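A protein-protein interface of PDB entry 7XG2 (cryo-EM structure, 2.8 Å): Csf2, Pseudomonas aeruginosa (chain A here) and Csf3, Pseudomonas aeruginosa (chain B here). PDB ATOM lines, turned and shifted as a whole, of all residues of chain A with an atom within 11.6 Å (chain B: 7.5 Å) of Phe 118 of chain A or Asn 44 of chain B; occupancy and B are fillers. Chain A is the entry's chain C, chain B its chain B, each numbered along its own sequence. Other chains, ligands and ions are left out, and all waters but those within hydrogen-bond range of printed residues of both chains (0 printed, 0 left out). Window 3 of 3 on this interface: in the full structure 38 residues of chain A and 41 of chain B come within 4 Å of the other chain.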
ATOM      1  N   VAL A 114      10.101 -29.383  -2.698  1.00  0.00           N
ATOM      2  CA  VAL A 114      10.978 -30.532  -3.061  1.00  0.00           C
ATOM      3  C   VAL A 114      11.856 -30.071  -4.225  1.00  0.00           C
ATOM      4  O   VAL A 114      11.294 -29.676  -5.262  1.00  0.00           O
ATOM      5  CB  VAL A 114      10.153 -31.779  -3.435  1.00  0.00           C
ATOM      6  CG1 VAL A 114      10.977 -32.795  -4.211  1.00  0.00           C
ATOM      7  CG2 VAL A 114       9.518 -32.424  -2.214  1.00  0.00           C
ATOM      8  N   PRO A 115      13.201 -30.105  -4.105  1.00  0.00           N
ATOM      9  CA  PRO A 115      14.079 -29.659  -5.182  1.00  0.00           C
ATOM     10  C   PRO A 115      14.290 -30.791  -6.196  1.00  0.00           C
ATOM     11  O   PRO A 115      14.625 -31.887  -5.786  1.00  0.00           O
ATOM     12  CB  PRO A 115      15.385 -29.380  -4.429  1.00  0.00           C
ATOM     13  CG  PRO A 115      15.396 -30.429  -3.342  1.00  0.00           C
ATOM     14  CD  PRO A 115      13.944 -30.578  -2.935  1.00  0.00           C
ATOM     15  N   SER A 116      14.086 -30.494  -7.481  1.00  0.00           N
ATOM     16  CA  SER A 116      14.270 -31.510  -8.549  1.00  0.00           C
ATOM     17  C   SER A 116      15.384 -31.055  -9.496  1.00  0.00           C
ATOM     18  O   SER A 116      15.307 -29.914  -9.991  1.00  0.00           O
ATOM     19  CB  SER A 116      12.979 -31.750  -9.287  1.00  0.00           C
ATOM     20  OG  SER A 116      12.356 -30.522  -9.629  1.00  0.00           O
ATOM     21  N   SER A 117      16.373 -31.921  -9.737  1.00  0.00           N
ATOM     22  CA  SER A 117      17.491 -31.587 -10.656  1.00  0.00           C
ATOM     23  C   SER A 117      16.965 -31.520 -12.093  1.00  0.00           C
ATOM     24  O   SER A 117      16.017 -32.264 -12.409  1.00  0.00           O
ATOM     25  CB  SER A 117      18.629 -32.566 -10.527  1.00  0.00           C
ATOM     26  OG  SER A 117      18.257 -33.838 -11.035  1.00  0.00           O
ATOM     27  N   PHE A 118      17.538 -30.641 -12.917  1.00  0.00           N
ATOM     28  CA  PHE A 118      17.074 -30.503 -14.296  1.00  0.00           C
ATOM     29  C   PHE A 118      17.073 -31.838 -15.031  1.00  0.00           C
ATOM     30  O   PHE A 118      16.231 -32.069 -15.909  1.00  0.00           O
ATOM     31  CB  PHE A 118      17.940 -29.481 -15.026  1.00  0.00           C
ATOM     32  CG  PHE A 118      18.108 -28.196 -14.276  1.00  0.00           C
ATOM     33  CD1 PHE A 118      17.001 -27.508 -13.803  1.00  0.00           C
ATOM     34  CD2 PHE A 118      19.371 -27.692 -14.014  1.00  0.00           C
ATOM     35  CE1 PHE A 118      17.149 -26.326 -13.103  1.00  0.00           C
ATOM     36  CE2 PHE A 118      19.526 -26.511 -13.312  1.00  0.00           C
ATOM     37  CZ  PHE A 118      18.412 -25.829 -12.856  1.00  0.00           C
ATOM     38  N   ASP A 119      18.006 -32.729 -14.685  1.00  0.00           N
ATOM     39  CA  ASP A 119      18.034 -34.056 -15.296  1.00  0.00           C
ATOM     40  C   ASP A 119      16.815 -34.873 -14.889  1.00  0.00           C
ATOM     41  O   ASP A 119      16.168 -35.503 -15.736  1.00  0.00           O
ATOM     42  CB  ASP A 119      19.327 -34.779 -14.914  1.00  0.00           C
ATOM     43  CG  ASP A 119      19.529 -36.077 -15.690  1.00  0.00           C
ATOM     44  OD1 ASP A 119      18.909 -37.101 -15.333  1.00  0.00           O
ATOM     45  OD2 ASP A 119      20.312 -36.072 -16.660  1.00  0.00           O
ATOM     46  N   GLU A 120      16.469 -34.860 -13.602  1.00  0.00           N
ATOM     47  CA  GLU A 120      15.289 -35.603 -13.185  1.00  0.00           C
ATOM     48  C   GLU A 120      14.001 -34.900 -13.598  1.00  0.00           C
ATOM     49  O   GLU A 120      12.999 -35.577 -13.833  1.00  0.00           O
ATOM     50  CB  GLU A 120      15.331 -35.883 -11.678  1.00  0.00           C
ATOM     51  CG  GLU A 120      15.168 -34.694 -10.761  1.00  0.00           C
ATOM     52  CD  GLU A 120      15.502 -35.042  -9.325  1.00  0.00           C
ATOM     53  OE1 GLU A 120      15.395 -36.230  -8.960  1.00  0.00           O
ATOM     54  OE2 GLU A 120      15.886 -34.132  -8.562  1.00  0.00           O
ATOM     55  N   ILE A 121      14.030 -33.568 -13.752  1.00  0.00           N
ATOM     56  CA  ILE A 121      12.917 -32.841 -14.367  1.00  0.00           C
ATOM     57  C   ILE A 121      12.694 -33.330 -15.794  1.00  0.00           C
ATOM     58  O   ILE A 121      11.555 -33.558 -16.221  1.00  0.00           O
ATOM     59  CB  ILE A 121      13.177 -31.320 -14.311  1.00  0.00           C
ATOM     60  CG1 ILE A 121      12.783 -30.753 -12.949  1.00  0.00           C
ATOM     61  CG2 ILE A 121      12.439 -30.560 -15.410  1.00  0.00           C
ATOM     62  CD1 ILE A 121      13.124 -29.293 -12.772  1.00  0.00           C
ATOM     63  N   ALA A 122      13.787 -33.556 -16.529  1.00  0.00           N
ATOM     64  CA  ALA A 122      13.693 -34.083 -17.888  1.00  0.00           C
ATOM     65  C   ALA A 122      13.166 -35.513 -17.911  1.00  0.00           C
ATOM     66  O   ALA A 122      12.361 -35.870 -18.779  1.00  0.00           O
ATOM     67  CB  ALA A 122      15.057 -34.019 -18.567  1.00  0.00           C
ATOM     68  N   THR A 123      13.630 -36.357 -16.981  1.00  0.00           N
ATOM     69  CA  THR A 123      13.202 -37.758 -17.003  1.00  0.00           C
ATOM     70  C   THR A 123      11.744 -37.915 -16.589  1.00  0.00           C
ATOM     71  O   THR A 123      11.033 -38.761 -17.143  1.00  0.00           O
ATOM     72  CB  THR A 123      14.081 -38.629 -16.101  1.00  0.00           C
ATOM     73  OG1 THR A 123      13.986 -38.176 -14.747  1.00  0.00           O
ATOM     74  CG2 THR A 123      15.531 -38.609 -16.564  1.00  0.00           C
ATOM     75  N   MET A 124      11.281 -37.125 -15.621  1.00  0.00           N
ATOM     76  CA  MET A 124       9.877 -37.179 -15.235  1.00  0.00           C
ATOM     77  C   MET A 124       8.983 -36.463 -16.239  1.00  0.00           C
ATOM     78  O   MET A 124       7.800 -36.793 -16.360  1.00  0.00           O
ATOM     79  CB  MET A 124       9.710 -36.595 -13.839  1.00  0.00           C
ATOM     80  CG  MET A 124      10.526 -37.326 -12.788  1.00  0.00           C
ATOM     81  SD  MET A 124      10.426 -36.512 -11.194  1.00  0.00           S
ATOM     82  CE  MET A 124      10.578 -34.809 -11.733  1.00  0.00           C
ATOM     83  N   ARG A 125       9.518 -35.485 -16.971  1.00  0.00           N
ATOM     84  CA  ARG A 125       8.745 -34.897 -18.057  1.00  0.00           C
ATOM     85  C   ARG A 125       8.669 -35.813 -19.269  1.00  0.00           C
ATOM     86  O   ARG A 125       7.801 -35.609 -20.124  1.00  0.00           O
ATOM     87  CB  ARG A 125       9.331 -33.546 -18.457  1.00  0.00           C
ATOM     88  CG  ARG A 125       8.752 -32.373 -17.685  1.00  0.00           C
ATOM     89  CD  ARG A 125       9.298 -31.053 -18.199  1.00  0.00           C
ATOM     90  NE  ARG A 125       8.440 -30.453 -19.213  1.00  0.00           N
ATOM     91  CZ  ARG A 125       7.808 -29.297 -19.064  1.00  0.00           C
ATOM     92  NH1 ARG A 125       7.922 -28.587 -17.956  1.00  0.00           N
ATOM     93  NH2 ARG A 125       7.046 -28.841 -20.055  1.00  0.00           N
ATOM     94  N   ALA A 126       9.548 -36.808 -19.364  1.00  0.00           N
ATOM     95  CA  ALA A 126       9.467 -37.838 -20.388  1.00  0.00           C
ATOM     96  C   ALA A 126       8.657 -39.044 -19.939  1.00  0.00           C
ATOM     97  O   ALA A 126       8.511 -39.998 -20.711  1.00  0.00           O
ATOM     98  CB  ALA A 126      10.872 -38.286 -20.800  1.00  0.00           C
ATOM     99  N   HIS A 127       8.154 -39.031 -18.710  1.00  0.00           N
ATOM    100  CA  HIS A 127       7.263 -40.082 -18.245  1.00  0.00           C
ATOM    101  C   HIS A 127       5.927 -39.984 -18.977  1.00  0.00           C
ATOM    102  O   HIS A 127       5.483 -38.875 -19.297  1.00  0.00           O
ATOM    103  CB  HIS A 127       7.062 -39.955 -16.736  1.00  0.00           C
ATOM    104  CG  HIS A 127       6.516 -41.184 -16.082  1.00  0.00           C
ATOM    105  ND1 HIS A 127       5.180 -41.339 -15.787  1.00  0.00           N
ATOM    106  CD2 HIS A 127       7.127 -42.316 -15.663  1.00  0.00           C
ATOM    107  CE1 HIS A 127       4.990 -42.514 -15.215  1.00  0.00           C
ATOM    108  NE2 HIS A 127       6.157 -43.126 -15.128  1.00  0.00           N
ATOM    109  N   ARG A 138       6.985 -31.165  -6.315  1.00  0.00           N
ATOM    110  CA  ARG A 138       7.901 -30.492  -7.220  1.00  0.00           C
ATOM    111  C   ARG A 138       7.229 -29.387  -8.019  1.00  0.00           C
ATOM    112  O   ARG A 138       7.909 -28.431  -8.409  1.00  0.00           O
ATOM    113  CB  ARG A 138       8.515 -31.517  -8.166  1.00  0.00           C
ATOM    114  CG  ARG A 138       9.271 -32.604  -7.443  1.00  0.00           C
ATOM    115  CD  ARG A 138       9.794 -33.609  -8.422  1.00  0.00           C
ATOM    116  NE  ARG A 138      10.160 -34.881  -7.814  1.00  0.00           N
ATOM    117  CZ  ARG A 138      11.376 -35.183  -7.382  1.00  0.00           C
ATOM    118  NH1 ARG A 138      12.381 -34.333  -7.498  1.00  0.00           N
ATOM    119  NH2 ARG A 138      11.590 -36.370  -6.825  1.00  0.00           N
ATOM    120  N   MET A 139       5.908 -29.492  -8.219  1.00  0.00           N
ATOM    121  CA  MET A 139       5.115 -28.620  -9.093  1.00  0.00           C
ATOM    122  C   MET A 139       5.716 -28.532 -10.493  1.00  0.00           C
ATOM    123  O   MET A 139       6.061 -27.457 -10.985  1.00  0.00           O
ATOM    124  CB  MET A 139       4.911 -27.232  -8.483  1.00  0.00           C
ATOM    125  CG  MET A 139       4.672 -27.258  -6.997  1.00  0.00           C
ATOM    126  SD  MET A 139       2.928 -27.566  -6.712  1.00  0.00           S
ATOM    127  CE  MET A 139       2.337 -25.903  -6.624  1.00  0.00           C
ATOM    128  N   LEU A 140       5.853 -29.694 -11.119  1.00  0.00           N
ATOM    129  CA  LEU A 140       6.375 -29.773 -12.473  1.00  0.00           C
ATOM    130  C   LEU A 140       5.359 -29.205 -13.453  1.00  0.00           C
ATOM    131  O   LEU A 140       4.158 -29.460 -13.331  1.00  0.00           O
ATOM    132  CB  LEU A 140       6.685 -31.227 -12.814  1.00  0.00           C
ATOM    133  CG  LEU A 140       7.877 -31.521 -13.711  1.00  0.00           C
ATOM    134  CD1 LEU A 140       9.126 -31.115 -12.974  1.00  0.00           C
ATOM    135  CD2 LEU A 140       7.913 -32.995 -14.062  1.00  0.00           C
ATOM    136  N   GLU A 141       5.832 -28.417 -14.414  1.00  0.00           N
ATOM    137  CA  GLU A 141       4.952 -27.976 -15.484  1.00  0.00           C
ATOM    138  C   GLU A 141       4.674 -29.138 -16.423  1.00  0.00           C
ATOM    139  O   GLU A 141       5.590 -29.838 -16.862  1.00  0.00           O
ATOM    140  CB  GLU A 141       5.563 -26.808 -16.254  1.00  0.00           C
ATOM    141  CG  GLU A 141       4.628 -26.219 -17.304  1.00  0.00           C
ATOM    142  CD  GLU A 141       5.347 -25.786 -18.565  1.00  0.00           C
ATOM    143  OE1 GLU A 141       6.580 -25.602 -18.519  1.00  0.00           O
ATOM    144  OE2 GLU A 141       4.673 -25.626 -19.604  1.00  0.00           O
ATOM    145  N   ARG A 143       3.428 -31.250 -19.801  1.00  0.00           N
ATOM    146  CA  ARG A 143       3.523 -31.121 -21.251  1.00  0.00           C
ATOM    147  C   ARG A 143       2.164 -30.827 -21.868  1.00  0.00           C
ATOM    148  O   ARG A 143       2.084 -30.423 -23.032  1.00  0.00           O
ATOM    149  CB  ARG A 143       4.105 -32.396 -21.862  1.00  0.00           C
ATOM    150  CG  ARG A 143       5.477 -32.794 -21.346  1.00  0.00           C
ATOM    151  CD  ARG A 143       6.554 -31.839 -21.818  1.00  0.00           C
ATOM    152  NE  ARG A 143       7.892 -32.378 -21.609  1.00  0.00           N
ATOM    153  CZ  ARG A 143       8.508 -33.198 -22.449  1.00  0.00           C
ATOM    154  NH1 ARG A 143       7.927 -33.612 -23.562  1.00  0.00           N
ATOM    155  NH2 ARG A 143       9.736 -33.617 -22.161  1.00  0.00           N
ATOM    156  N   ARG A 266       5.714 -30.321 -26.938  1.00  0.00           N
ATOM    157  CA  ARG A 266       6.849 -31.155 -27.342  1.00  0.00           C
ATOM    158  C   ARG A 266       6.839 -32.511 -26.644  1.00  0.00           C
ATOM    159  O   ARG A 266       7.744 -32.803 -25.853  1.00  0.00           O
ATOM    160  CB  ARG A 266       8.175 -30.444 -27.064  1.00  0.00           C
ATOM    161  CG  ARG A 266       8.296 -29.065 -27.680  1.00  0.00           C
ATOM    162  CD  ARG A 266       9.499 -28.343 -27.112  1.00  0.00           C
ATOM    163  NE  ARG A 266       9.133 -27.511 -25.973  1.00  0.00           N
ATOM    164  CZ  ARG A 266       9.430 -27.799 -24.714  1.00  0.00           C
ATOM    165  NH1 ARG A 266      10.077 -28.906 -24.392  1.00  0.00           N
ATOM    166  NH2 ARG A 266       9.057 -26.959 -23.753  1.00  0.00           N
ATOM    167  N   PHE A 341       8.515 -39.363  -7.939  1.00  0.00           N
ATOM    168  CA  PHE A 341       7.990 -38.080  -8.383  1.00  0.00           C
ATOM    169  C   PHE A 341       7.329 -37.343  -7.229  1.00  0.00           C
ATOM    170  O   PHE A 341       7.422 -36.113  -7.141  1.00  0.00           O
ATOM    171  CB  PHE A 341       7.002 -38.291  -9.531  1.00  0.00           C
ATOM    172  CG  PHE A 341       6.347 -37.029 -10.015  1.00  0.00           C
ATOM    173  CD1 PHE A 341       7.103 -35.898 -10.285  1.00  0.00           C
ATOM    174  CD2 PHE A 341       4.978 -36.969 -10.198  1.00  0.00           C
ATOM    175  CE1 PHE A 341       6.513 -34.739 -10.729  1.00  0.00           C
ATOM    176  CE2 PHE A 341       4.384 -35.806 -10.651  1.00  0.00           C
ATOM    177  CZ  PHE A 341       5.154 -34.694 -10.907  1.00  0.00           C
ATOM    178  N   VAL B  32      13.279 -20.209 -23.391  1.00  0.00           N
ATOM    179  CA  VAL B  32      13.512 -21.436 -22.632  1.00  0.00           C
ATOM    180  C   VAL B  32      12.836 -22.625 -23.309  1.00  0.00           C
ATOM    181  O   VAL B  32      13.422 -23.710 -23.412  1.00  0.00           O
ATOM    182  CB  VAL B  32      13.043 -21.240 -21.174  1.00  0.00           C
ATOM    183  CG1 VAL B  32      12.796 -22.564 -20.468  1.00  0.00           C
ATOM    184  CG2 VAL B  32      14.072 -20.443 -20.406  1.00  0.00           C
ATOM    185  N   ALA B  35      14.912 -23.487 -26.307  1.00  0.00           N
ATOM    186  CA  ALA B  35      16.114 -24.206 -25.898  1.00  0.00           C
ATOM    187  C   ALA B  35      15.794 -25.640 -25.495  1.00  0.00           C
ATOM    188  O   ALA B  35      16.612 -26.546 -25.693  1.00  0.00           O
ATOM    189  CB  ALA B  35      16.797 -23.467 -24.749  1.00  0.00           C
ATOM    190  N   ARG B  36      14.612 -25.862 -24.913  1.00  0.00           N
ATOM    191  CA  ARG B  36      14.170 -27.222 -24.624  1.00  0.00           C
ATOM    192  C   ARG B  36      13.871 -27.982 -25.907  1.00  0.00           C
ATOM    193  O   ARG B  36      14.041 -29.205 -25.969  1.00  0.00           O
ATOM    194  CB  ARG B  36      12.933 -27.203 -23.727  1.00  0.00           C
ATOM    195  CG  ARG B  36      13.184 -26.783 -22.298  1.00  0.00           C
ATOM    196  CD  ARG B  36      11.961 -27.061 -21.442  1.00  0.00           C
ATOM    197  NE  ARG B  36      11.798 -26.079 -20.377  1.00  0.00           N
ATOM    198  CZ  ARG B  36      12.425 -26.121 -19.211  1.00  0.00           C
ATOM    199  NH1 ARG B  36      13.280 -27.089 -18.920  1.00  0.00           N
ATOM    200  NH2 ARG B  36      12.186 -25.172 -18.311  1.00  0.00           N
ATOM    201  N   GLY B  40      17.193 -30.409 -25.748  1.00  0.00           N
ATOM    202  CA  GLY B  40      16.566 -31.393 -24.891  1.00  0.00           C
ATOM    203  C   GLY B  40      15.937 -30.775 -23.656  1.00  0.00           C
ATOM    204  O   GLY B  40      16.093 -29.593 -23.351  1.00  0.00           O
ATOM    205  N   ASP B  41      15.210 -31.614 -22.920  1.00  0.00           N
ATOM    206  CA  ASP B  41      14.531 -31.143 -21.720  1.00  0.00           C
ATOM    207  C   ASP B  41      15.495 -30.933 -20.557  1.00  0.00           C
ATOM    208  O   ASP B  41      15.191 -30.164 -19.638  1.00  0.00           O
ATOM    209  CB  ASP B  41      13.431 -32.128 -21.327  1.00  0.00           C
ATOM    210  CG  ASP B  41      12.195 -31.439 -20.784  1.00  0.00           C
ATOM    211  OD1 ASP B  41      12.330 -30.357 -20.174  1.00  0.00           O
ATOM    212  OD2 ASP B  41      11.087 -31.979 -20.973  1.00  0.00           O
ATOM    213  N   ALA B  42      16.655 -31.590 -20.580  1.00  0.00           N
ATOM    214  CA  ALA B  42      17.632 -31.496 -19.494  1.00  0.00           C
ATOM    215  C   ALA B  42      18.518 -30.275 -19.715  1.00  0.00           C
ATOM    216  O   ALA B  42      19.691 -30.369 -20.082  1.00  0.00           O
ATOM    217  CB  ALA B  42      18.460 -32.771 -19.403  1.00  0.00           C
ATOM    218  N   ILE B  43      17.935 -29.097 -19.490  1.00  0.00           N
ATOM    219  CA  ILE B  43      18.674 -27.844 -19.549  1.00  0.00           C
ATOM    220  C   ILE B  43      18.438 -27.079 -18.257  1.00  0.00           C
ATOM    221  O   ILE B  43      17.458 -27.298 -17.543  1.00  0.00           O
ATOM    222  CB  ILE B  43      18.286 -26.960 -20.762  1.00  0.00           C
ATOM    223  CG1 ILE B  43      16.835 -26.489 -20.649  1.00  0.00           C
ATOM    224  CG2 ILE B  43      18.534 -27.681 -22.080  1.00  0.00           C
ATOM    225  CD1 ILE B  43      16.548 -25.215 -21.403  1.00  0.00           C
ATOM    226  N   ASN B  44      19.373 -26.184 -17.953  1.00  0.00           N
ATOM    227  CA  ASN B  44      19.145 -25.156 -16.952  1.00  0.00           C
ATOM    228  C   ASN B  44      18.336 -24.065 -17.631  1.00  0.00           C
ATOM    229  O   ASN B  44      18.809 -23.485 -18.621  1.00  0.00           O
ATOM    230  CB  ASN B  44      20.463 -24.602 -16.428  1.00  0.00           C
ATOM    231  CG  ASN B  44      20.300 -23.727 -15.188  1.00  0.00           C
ATOM    232  OD1 ASN B  44      19.190 -23.382 -14.784  1.00  0.00           O
ATOM    233  ND2 ASN B  44      21.421 -23.367 -14.579  1.00  0.00           N
ATOM    234  N   PRO B  45      17.121 -23.767 -17.169  1.00  0.00           N
ATOM    235  CA  PRO B  45      16.349 -22.681 -17.787  1.00  0.00           C
ATOM    236  C   PRO B  45      16.929 -21.303 -17.534  1.00  0.00           C
ATOM    237  O   PRO B  45      16.623 -20.373 -18.288  1.00  0.00           O
ATOM    238  CB  PRO B  45      14.962 -22.833 -17.148  1.00  0.00           C
ATOM    239  CG  PRO B  45      14.940 -24.210 -16.566  1.00  0.00           C
ATOM    240  CD  PRO B  45      16.342 -24.481 -16.147  1.00  0.00           C
ATOM    241  N   ARG B  46      17.755 -21.137 -16.505  1.00  0.00           N
ATOM    242  CA  ARG B  46      18.361 -19.843 -16.228  1.00  0.00           C
ATOM    243  C   ARG B  46      19.561 -19.537 -17.112  1.00  0.00           C
ATOM    244  O   ARG B  46      20.038 -18.398 -17.096  1.00  0.00           O
ATOM    245  CB  ARG B  46      18.766 -19.762 -14.759  1.00  0.00           C
ATOM    246  CG  ARG B  46      17.630 -20.059 -13.811  1.00  0.00           C
ATOM    247  CD  ARG B  46      17.584 -19.031 -12.708  1.00  0.00           C
ATOM    248  NE  ARG B  46      16.379 -19.146 -11.899  1.00  0.00           N
ATOM    249  CZ  ARG B  46      16.199 -18.517 -10.748  1.00  0.00           C
ATOM    250  NH1 ARG B  46      17.138 -17.740 -10.234  1.00  0.00           N
ATOM    251  NH2 ARG B  46      15.055 -18.678 -10.092  1.00  0.00           N
ATOM    252  N   ASP B  47      20.072 -20.515 -17.863  1.00  0.00           N
ATOM    253  CA  ASP B  47      21.132 -20.215 -18.823  1.00  0.00           C
ATOM    254  C   ASP B  47      20.598 -19.405 -19.995  1.00  0.00           C
ATOM    255  O   ASP B  47      21.272 -18.492 -20.484  1.00  0.00           O
ATOM    256  CB  ASP B  47      21.783 -21.499 -19.336  1.00  0.00           C
ATOM    257  CG  ASP B  47      22.558 -22.235 -18.267  1.00  0.00           C
ATOM    258  OD1 ASP B  47      22.949 -21.598 -17.266  1.00  0.00           O
ATOM    259  OD2 ASP B  47      22.772 -23.454 -18.429  1.00  0.00           O
ATOM    260  N   TYR B  48      19.386 -19.716 -20.453  1.00  0.00           N
ATOM    261  CA  TYR B  48      18.878 -19.171 -21.701  1.00  0.00           C
ATOM    262  C   TYR B  48      17.736 -18.185 -21.519  1.00  0.00           C
ATOM    263  O   TYR B  48      17.308 -17.586 -22.507  1.00  0.00           O
ATOM    264  CB  TYR B  48      18.405 -20.280 -22.670  1.00  0.00           C
ATOM    265  CG  TYR B  48      19.202 -21.580 -22.751  1.00  0.00           C
ATOM    266  CD1 TYR B  48      19.171 -22.537 -21.733  1.00  0.00           C
ATOM    267  CD2 TYR B  48      20.013 -21.832 -23.850  1.00  0.00           C
ATOM    268  CE1 TYR B  48      19.906 -23.702 -21.821  1.00  0.00           C
ATOM    269  CE2 TYR B  48      20.753 -22.996 -23.942  1.00  0.00           C
ATOM    270  CZ  TYR B  48      20.693 -23.926 -22.928  1.00  0.00           C
ATOM    271  OH  TYR B  48      21.428 -25.085 -23.020  1.00  0.00           O
ATOM    272  N   HIS B  49      17.244 -17.977 -20.298  1.00  0.00           N
ATOM    273  CA  HIS B  49      16.124 -17.062 -20.111  1.00  0.00           C
ATOM    274  C   HIS B  49      16.521 -15.597 -20.249  1.00  0.00           C
ATOM    275  O   HIS B  49      15.635 -14.741 -20.334  1.00  0.00           O
ATOM    276  CB  HIS B  49      15.456 -17.314 -18.754  1.00  0.00           C
ATOM    277  CG  HIS B  49      16.187 -16.726 -17.587  1.00  0.00           C
ATOM    278  ND1 HIS B  49      17.558 -16.763 -17.465  1.00  0.00           N
ATOM    279  CD2 HIS B  49      15.728 -16.102 -16.477  1.00  0.00           C
ATOM    280  CE1 HIS B  49      17.913 -16.179 -16.334  1.00  0.00           C
ATOM    281  NE2 HIS B  49      16.821 -15.771 -15.715  1.00  0.00           N
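The guanidinium group (NE) of Arg 125 of chain A lies within salt-bridge range of the side-chain carboxylate (OD2) of Asp 41 of chain B (3.5 Å). The side-chain carboxylate (OD2) of Asp 41 of chain B is in salt-bridge range of the guanidinium group (NH2) of Arg 143 of chain A, 2.4 Å away.
Of the 13 printed residues of chain B, 6 touch a printed residue of chain A. Of the 21 printed residues of chain A, 5 touch a printed residue of chain B. Printed residues of chain A that touch a printed residue of chain B: Phe 118, Ala 122, Arg 125, Arg 143 and Arg 266. Among the printed residues, Asp or Glu carboxylates within 4 Å of a Lys or Arg side-chain nitrogen of the other chain: Arg 125 of chain A with Asp 41 of chain B and Arg 143 of chain A with Asp 41 of chain B.
Phe 118 of chain A touches just these residues of chain B: Ala 42, Ile 43, Asn 44 and Pro 45. Asn 44 of chain B touches one residue of chain A. Printed residues of chain A within 4 Å of Ala 42 of chain B: Phe 118 and Ala 122. No residue of chain A comes within 4 Å of Asp 47 of chain B. Tyr 48 of chain B touches none of the printed residues of chain A. Printed residues of chain B within 4 Å of Ala 122 of chain A: Asp 41 and Ala 42. Printed residues of chain B within 4 Å of Arg 125 of chain A: Asp 41. Printed residues of chain A within 4 Å of Arg 36 of chain B: Arg 266. Of the printed residues of chain B, Arg 143 of chain A touches Asp 41. Arg 46 of chain B touches none of the printed residues of chain A. Arg 138 of chain A touches none of the printed residues of chain B. The nearest residue of chain B that does not touch Phe 118 of chain A is Asp 41 of chain B (4.3 Å). The nearest residue of chain A that does not touch Asn 44 of chain B is Asp 119 of chain A (7.4 Å).
O of Phe 118 of chain A touches CA of Ala 42 of chain B, 3.9 Å away. CB of Phe 118 of chain A touches O of Ile 43 of chain B (3.4 Å). OD1 of Asn 44 of chain B touches CZ of Phe 118 of chain A, 3.2 Å away. Phe 118 of chain A touches Pro 45 of chain B (CE1 to CD, 3.6 Å). C of Asp 41 of chain B touches CB of Ala 122 of chain A (3.7 Å). Ala 122 of chain A touches Ala 42 of chain B (CB to N, 3.5 Å). Arg 266 of chain A touches Arg 36 of chain B (NH1 to CB, 3.4 Å).
The side-chain carboxylate (OD1) of Asp 41 of chain B is in salt-bridge range of the guanidinium group (NH1) of Arg 36 of chain B. The side-chain amide oxygen (OD1) of Asn 44 of chain B is in hydrogen-bond range of the backbone NH (N) of Arg 46 of chain B. The guanidinium group of Arg 125 of chain A lies within salt-bridge range of the side-chain carboxylate of Glu 141 of chain A, 3.3 Å away. O of Arg 125 of chain A sits close to NH2 of Arg 143 of chain A, 3.4 Å away. The guanidinium group of Arg 143 of chain A lies within hydrogen-bond range of the backbone carbonyl oxygen of Arg 266 of chain A, at 2.4 Å.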
